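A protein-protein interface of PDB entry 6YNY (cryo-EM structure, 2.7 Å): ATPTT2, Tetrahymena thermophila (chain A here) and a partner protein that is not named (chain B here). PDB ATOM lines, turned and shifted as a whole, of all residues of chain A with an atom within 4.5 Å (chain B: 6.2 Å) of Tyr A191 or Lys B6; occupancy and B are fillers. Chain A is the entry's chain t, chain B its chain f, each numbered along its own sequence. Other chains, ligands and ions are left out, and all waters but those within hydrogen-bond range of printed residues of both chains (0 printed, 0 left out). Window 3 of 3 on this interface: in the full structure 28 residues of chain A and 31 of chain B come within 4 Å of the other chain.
OH of Tyr A191 is in hydrogen-bond range of OD2 of Asp B10, at 2.9 Å.
The backbone carbonyl oxygen of Arg A188 lies within hydrogen-bond range of the side-chain hydroxyl of Ser A192, 3.3 Å away.
Met A187 touches Trp B13 (SD to CZ2, 3.4 Å).
CD2 of Leu B3 touches CB of Arg A188, 3.97 Å away.
CG of Arg A188 touches CE of Met B7, 3.7 Å away.
Tyr A191 touches Lys B6 (OH to CE, 3.2 Å).
CB of Met B7 touches CG of Tyr A191, at 3.5 Å.
Trp B13 touches Tyr A191 (CD2 to CD1, 3.7 Å).
CZ of Phe A443 touches CE3 of Trp B13, at 3.4 Å.
Of chain B, only Lys B6, Met B7, Asp B10 and Trp B13 come within 4 Å of Tyr A191.
Of the printed residues of chain A, Trp B13 touches Met A187 (3.4 Å), Tyr A191 (3.7 Å) and Phe A443 (3.4 Å).
Of the printed residues of chain A, Asp B10 touches Tyr A191 (2.9 Å).
Printed residues of chain B within 4 Å of Arg A188: Leu B3 (3.97 Å) and Met B7 (3.7 Å).
Of the printed residues of chain B, Phe A443 touches Trp B13.
Ser A192 touches none of the printed residues of chain B.
Phe A189 touches none of the printed residues of chain B.
The nearest printed residue of chain A that does not touch Met B7 is Met A187 (4.1 Å).
Of the 9 printed residues of chain A, 4 touch a printed residue of chain B.
Printed residues of chain A that touch a printed residue of chain B: Met A187, Arg A188, Tyr A191 and Phe A443.
Hydrophobic or aromatic side chains of chain A that line the printed part of chain B: Met A187, Tyr A191 and Phe A443.
Among the printed residues, 8 pairs touch across the chains.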
ATOM      1  N   MET A 187      23.430   6.745  13.944  1.00  0.00           N
ATOM      2  CA  MET A 187      23.258   7.926  13.111  1.00  0.00           C
ATOM      3  C   MET A 187      24.280   8.995  13.468  1.00  0.00           C
ATOM      4  O   MET A 187      24.764   9.717  12.589  1.00  0.00           O
ATOM      5  CB  MET A 187      21.834   8.455  13.262  1.00  0.00           C
ATOM      6  CG  MET A 187      21.311   9.230  12.073  1.00  0.00           C
ATOM      7  SD  MET A 187      21.490   8.362  10.501  1.00  0.00           S
ATOM      8  CE  MET A 187      21.024   6.702  10.961  1.00  0.00           C
ATOM      9  N   ARG A 188      24.620   9.114  14.751  1.00  0.00           N
ATOM     10  CA  ARG A 188      25.668  10.044  15.154  1.00  0.00           C
ATOM     11  C   ARG A 188      27.032   9.563  14.686  1.00  0.00           C
ATOM     12  O   ARG A 188      27.860  10.364  14.237  1.00  0.00           O
ATOM     13  CB  ARG A 188      25.652  10.224  16.667  1.00  0.00           C
ATOM     14  CG  ARG A 188      24.384  10.854  17.185  1.00  0.00           C
ATOM     15  CD  ARG A 188      24.498  11.230  18.643  1.00  0.00           C
ATOM     16  NE  ARG A 188      24.668  10.067  19.504  1.00  0.00           N
ATOM     17  CZ  ARG A 188      23.670   9.365  20.025  1.00  0.00           C
ATOM     18  NH1 ARG A 188      23.931   8.327  20.797  1.00  0.00           N
ATOM     19  NH2 ARG A 188      22.413   9.695  19.783  1.00  0.00           N
ATOM     20  N   PHE A 189      27.286   8.258  14.783  1.00  0.00           N
ATOM     21  CA  PHE A 189      28.528   7.705  14.259  1.00  0.00           C
ATOM     22  C   PHE A 189      28.660   8.001  12.773  1.00  0.00           C
ATOM     23  O   PHE A 189      29.712   8.450  12.307  1.00  0.00           O
ATOM     24  CB  PHE A 189      28.573   6.200  14.518  1.00  0.00           C
ATOM     25  CG  PHE A 189      29.765   5.519  13.927  1.00  0.00           C
ATOM     26  CD1 PHE A 189      30.930   5.384  14.654  1.00  0.00           C
ATOM     27  CD2 PHE A 189      29.721   5.009  12.647  1.00  0.00           C
ATOM     28  CE1 PHE A 189      32.024   4.759  14.113  1.00  0.00           C
ATOM     29  CE2 PHE A 189      30.811   4.384  12.104  1.00  0.00           C
ATOM     30  CZ  PHE A 189      31.965   4.258  12.840  1.00  0.00           C
ATOM     31  N   MET A 190      27.594   7.754  12.014  1.00  0.00           N
ATOM     32  CA  MET A 190      27.611   8.057  10.590  1.00  0.00           C
ATOM     33  C   MET A 190      27.856   9.537  10.341  1.00  0.00           C
ATOM     34  O   MET A 190      28.512   9.902   9.360  1.00  0.00           O
ATOM     35  CB  MET A 190      26.291   7.616   9.965  1.00  0.00           C
ATOM     36  CG  MET A 190      26.074   6.119  10.015  1.00  0.00           C
ATOM     37  SD  MET A 190      24.399   5.609   9.613  1.00  0.00           S
ATOM     38  CE  MET A 190      24.301   6.147   7.919  1.00  0.00           C
ATOM     39  N   TYR A 191      27.342  10.400  11.216  1.00  0.00           N
ATOM     40  CA  TYR A 191      27.569  11.832  11.070  1.00  0.00           C
ATOM     41  C   TYR A 191      29.008  12.194  11.406  1.00  0.00           C
ATOM     42  O   TYR A 191      29.679  12.897  10.642  1.00  0.00           O
ATOM     43  CB  TYR A 191      26.600  12.602  11.962  1.00  0.00           C
ATOM     44  CG  TYR A 191      26.823  14.089  11.954  1.00  0.00           C
ATOM     45  CD1 TYR A 191      26.356  14.872  10.914  1.00  0.00           C
ATOM     46  CD2 TYR A 191      27.501  14.713  12.989  1.00  0.00           C
ATOM     47  CE1 TYR A 191      26.558  16.230  10.903  1.00  0.00           C
ATOM     48  CE2 TYR A 191      27.706  16.070  12.985  1.00  0.00           C
ATOM     49  CZ  TYR A 191      27.232  16.825  11.939  1.00  0.00           C
ATOM     50  OH  TYR A 191      27.429  18.182  11.921  1.00  0.00           O
ATOM     51  N   SER A 192      29.500  11.723  12.553  1.00  0.00           N
ATOM     52  CA  SER A 192      30.870  12.023  12.947  1.00  0.00           C
ATOM     53  C   SER A 192      31.868  11.492  11.932  1.00  0.00           C
ATOM     54  O   SER A 192      32.909  12.115  11.697  1.00  0.00           O
ATOM     55  CB  SER A 192      31.157  11.428  14.321  1.00  0.00           C
ATOM     56  OG  SER A 192      31.162  10.016  14.262  1.00  0.00           O
ATOM     57  N   GLN A 193      31.568  10.352  11.322  1.00  0.00           N
ATOM     58  CA  GLN A 193      32.426   9.761  10.311  1.00  0.00           C
ATOM     59  C   GLN A 193      32.086  10.230   8.905  1.00  0.00           C
ATOM     60  O   GLN A 193      32.708   9.765   7.946  1.00  0.00           O
ATOM     61  CB  GLN A 193      32.328   8.239  10.378  1.00  0.00           C
ATOM     62  CG  GLN A 193      33.661   7.541  10.465  1.00  0.00           C
ATOM     63  CD  GLN A 193      34.374   7.819  11.767  1.00  0.00           C
ATOM     64  OE1 GLN A 193      33.764   8.246  12.745  1.00  0.00           O
ATOM     65  NE2 GLN A 193      35.676   7.578  11.788  1.00  0.00           N
ATOM     66  N   LYS A 194      31.116  11.131   8.760  1.00  0.00           N
ATOM     67  CA  LYS A 194      30.746  11.690   7.462  1.00  0.00           C
ATOM     68  C   LYS A 194      30.268  10.603   6.503  1.00  0.00           C
ATOM     69  O   LYS A 194      30.771  10.454   5.388  1.00  0.00           O
ATOM     70  CB  LYS A 194      31.906  12.486   6.866  1.00  0.00           C
ATOM     71  CG  LYS A 194      32.259  13.713   7.677  1.00  0.00           C
ATOM     72  CD  LYS A 194      33.449  14.444   7.103  1.00  0.00           C
ATOM     73  CE  LYS A 194      33.782  15.674   7.925  1.00  0.00           C
ATOM     74  NZ  LYS A 194      35.007  16.359   7.433  1.00  0.00           N
ATOM     75  N   PHE A 443      28.305  14.778   1.961  1.00  0.00           N
ATOM     76  CA  PHE A 443      29.597  15.215   2.458  1.00  0.00           C
ATOM     77  C   PHE A 443      30.639  15.356   1.357  1.00  0.00           C
ATOM     78  O   PHE A 443      31.818  15.561   1.662  1.00  0.00           O
ATOM     79  CB  PHE A 443      30.084  14.246   3.531  1.00  0.00           C
ATOM     80  CG  PHE A 443      29.176  14.172   4.717  1.00  0.00           C
ATOM     81  CD1 PHE A 443      29.095  15.225   5.604  1.00  0.00           C
ATOM     82  CD2 PHE A 443      28.401  13.055   4.943  1.00  0.00           C
ATOM     83  CE1 PHE A 443      28.259  15.164   6.693  1.00  0.00           C
ATOM     84  CE2 PHE A 443      27.564  12.988   6.033  1.00  0.00           C
ATOM     85  CZ  PHE A 443      27.494  14.046   6.909  1.00  0.00           C
ATOM     86  N   SER B   2      25.454  17.139  22.839  1.00  0.00           N
ATOM     87  CA  SER B   2      25.937  18.180  21.940  1.00  0.00           C
ATOM     88  C   SER B   2      26.016  17.663  20.513  1.00  0.00           C
ATOM     89  O   SER B   2      25.519  18.299  19.583  1.00  0.00           O
ATOM     90  CB  SER B   2      27.308  18.684  22.389  1.00  0.00           C
ATOM     91  OG  SER B   2      28.258  17.633  22.400  1.00  0.00           O
ATOM     92  N   LEU B   3      26.652  16.501  20.345  1.00  0.00           N
ATOM     93  CA  LEU B   3      26.763  15.910  19.017  1.00  0.00           C
ATOM     94  C   LEU B   3      25.391  15.655  18.412  1.00  0.00           C
ATOM     95  O   LEU B   3      25.232  15.700  17.187  1.00  0.00           O
ATOM     96  CB  LEU B   3      27.561  14.612  19.086  1.00  0.00           C
ATOM     97  CG  LEU B   3      27.884  13.963  17.743  1.00  0.00           C
ATOM     98  CD1 LEU B   3      28.767  14.866  16.910  1.00  0.00           C
ATOM     99  CD2 LEU B   3      28.549  12.618  17.947  1.00  0.00           C
ATOM    100  N   HIS B   4      24.392  15.383  19.251  1.00  0.00           N
ATOM    101  CA  HIS B   4      23.037  15.188  18.756  1.00  0.00           C
ATOM    102  C   HIS B   4      22.492  16.475  18.153  1.00  0.00           C
ATOM    103  O   HIS B   4      21.991  16.484  17.023  1.00  0.00           O
ATOM    104  CB  HIS B   4      22.140  14.695  19.888  1.00  0.00           C
ATOM    105  CG  HIS B   4      20.724  14.448  19.476  1.00  0.00           C
ATOM    106  ND1 HIS B   4      19.707  15.342  19.729  1.00  0.00           N
ATOM    107  CD2 HIS B   4      20.155  13.404  18.829  1.00  0.00           C
ATOM    108  CE1 HIS B   4      18.573  14.860  19.256  1.00  0.00           C
ATOM    109  NE2 HIS B   4      18.817  13.686  18.704  1.00  0.00           N
ATOM    110  N   GLU B   5      22.579  17.578  18.899  1.00  0.00           N
ATOM    111  CA  GLU B   5      22.124  18.862  18.382  1.00  0.00           C
ATOM    112  C   GLU B   5      23.046  19.375  17.285  1.00  0.00           C
ATOM    113  O   GLU B   5      22.591  20.057  16.360  1.00  0.00           O
ATOM    114  CB  GLU B   5      22.037  19.877  19.520  1.00  0.00           C
ATOM    115  CG  GLU B   5      21.111  19.458  20.649  1.00  0.00           C
ATOM    116  CD  GLU B   5      21.233  20.348  21.868  1.00  0.00           C
ATOM    117  OE1 GLU B   5      22.026  21.312  21.827  1.00  0.00           O
ATOM    118  OE2 GLU B   5      20.539  20.079  22.872  1.00  0.00           O
ATOM    119  N   LYS B   6      24.339  19.059  17.372  1.00  0.00           N
ATOM    120  CA  LYS B   6      25.286  19.494  16.354  1.00  0.00           C
ATOM    121  C   LYS B   6      24.862  19.022  14.968  1.00  0.00           C
ATOM    122  O   LYS B   6      24.904  19.793  14.004  1.00  0.00           O
ATOM    123  CB  LYS B   6      26.684  18.987  16.711  1.00  0.00           C
ATOM    124  CG  LYS B   6      27.671  18.864  15.559  1.00  0.00           C
ATOM    125  CD  LYS B   6      27.934  20.183  14.871  1.00  0.00           C
ATOM    126  CE  LYS B   6      29.110  20.063  13.919  1.00  0.00           C
ATOM    127  NZ  LYS B   6      29.251  21.257  13.041  1.00  0.00           N
ATOM    128  N   MET B   7      24.446  17.761  14.848  1.00  0.00           N
ATOM    129  CA  MET B   7      24.072  17.238  13.540  1.00  0.00           C
ATOM    130  C   MET B   7      22.671  17.679  13.135  1.00  0.00           C
ATOM    131  O   MET B   7      22.403  17.851  11.942  1.00  0.00           O
ATOM    132  CB  MET B   7      24.174  15.714  13.521  1.00  0.00           C
ATOM    133  CG  MET B   7      23.186  14.994  14.388  1.00  0.00           C
ATOM    134  SD  MET B   7      23.394  13.210  14.263  1.00  0.00           S
ATOM    135  CE  MET B   7      21.917  12.652  15.095  1.00  0.00           C
ATOM    136  N   GLN B   8      21.771  17.861  14.103  1.00  0.00           N
ATOM    137  CA  GLN B   8      20.444  18.373  13.779  1.00  0.00           C
ATOM    138  C   GLN B   8      20.535  19.738  13.115  1.00  0.00           C
ATOM    139  O   GLN B   8      19.827  20.013  12.140  1.00  0.00           O
ATOM    140  CB  GLN B   8      19.593  18.465  15.043  1.00  0.00           C
ATOM    141  CG  GLN B   8      19.075  17.139  15.554  1.00  0.00           C
ATOM    142  CD  GLN B   8      18.143  17.313  16.734  1.00  0.00           C
ATOM    143  OE1 GLN B   8      18.269  18.264  17.505  1.00  0.00           O
ATOM    144  NE2 GLN B   8      17.191  16.401  16.874  1.00  0.00           N
ATOM    145  N   THR B   9      21.402  20.608  13.633  1.00  0.00           N
ATOM    146  CA  THR B   9      21.536  21.942  13.062  1.00  0.00           C
ATOM    147  C   THR B   9      22.284  21.912  11.738  1.00  0.00           C
ATOM    148  O   THR B   9      22.069  22.782  10.887  1.00  0.00           O
ATOM    149  CB  THR B   9      22.255  22.864  14.043  1.00  0.00           C
ATOM    150  OG1 THR B   9      21.538  22.903  15.283  1.00  0.00           O
ATOM    151  CG2 THR B   9      22.361  24.270  13.476  1.00  0.00           C
ATOM    152  N   ASP B  10      23.163  20.930  11.544  1.00  0.00           N
ATOM    153  CA  ASP B  10      23.971  20.879  10.335  1.00  0.00           C
ATOM    154  C   ASP B  10      23.074  20.852   9.107  1.00  0.00           C
ATOM    155  O   ASP B  10      22.190  20.001   8.985  1.00  0.00           O
ATOM    156  CB  ASP B  10      24.882  19.657  10.354  1.00  0.00           C
ATOM    157  CG  ASP B  10      25.894  19.667   9.226  1.00  0.00           C
ATOM    158  OD1 ASP B  10      25.855  20.598   8.396  1.00  0.00           O
ATOM    159  OD2 ASP B  10      26.735  18.746   9.170  1.00  0.00           O
ATOM    160  N   TRP B  13      23.486  17.566   6.893  1.00  0.00           N
ATOM    161  CA  TRP B  13      22.855  16.344   7.376  1.00  0.00           C
ATOM    162  C   TRP B  13      21.360  16.329   7.095  1.00  0.00           C
ATOM    163  O   TRP B  13      20.792  15.263   6.838  1.00  0.00           O
ATOM    164  CB  TRP B  13      23.112  16.185   8.870  1.00  0.00           C
ATOM    165  CG  TRP B  13      22.795  14.833   9.395  1.00  0.00           C
ATOM    166  CD1 TRP B  13      21.873  14.523  10.342  1.00  0.00           C
ATOM    167  CD2 TRP B  13      23.402  13.600   9.007  1.00  0.00           C
ATOM    168  NE1 TRP B  13      21.866  13.172  10.572  1.00  0.00           N
ATOM    169  CE2 TRP B  13      22.800  12.583   9.765  1.00  0.00           C
ATOM    170  CE3 TRP B  13      24.398  13.256   8.091  1.00  0.00           C
ATOM    171  CZ2 TRP B  13      23.154  11.249   9.632  1.00  0.00           C
ATOM    172  CZ3 TRP B  13      24.750  11.932   7.964  1.00  0.00           C
ATOM    173  CH2 TRP B  13      24.131  10.945   8.730  1.00  0.00           C
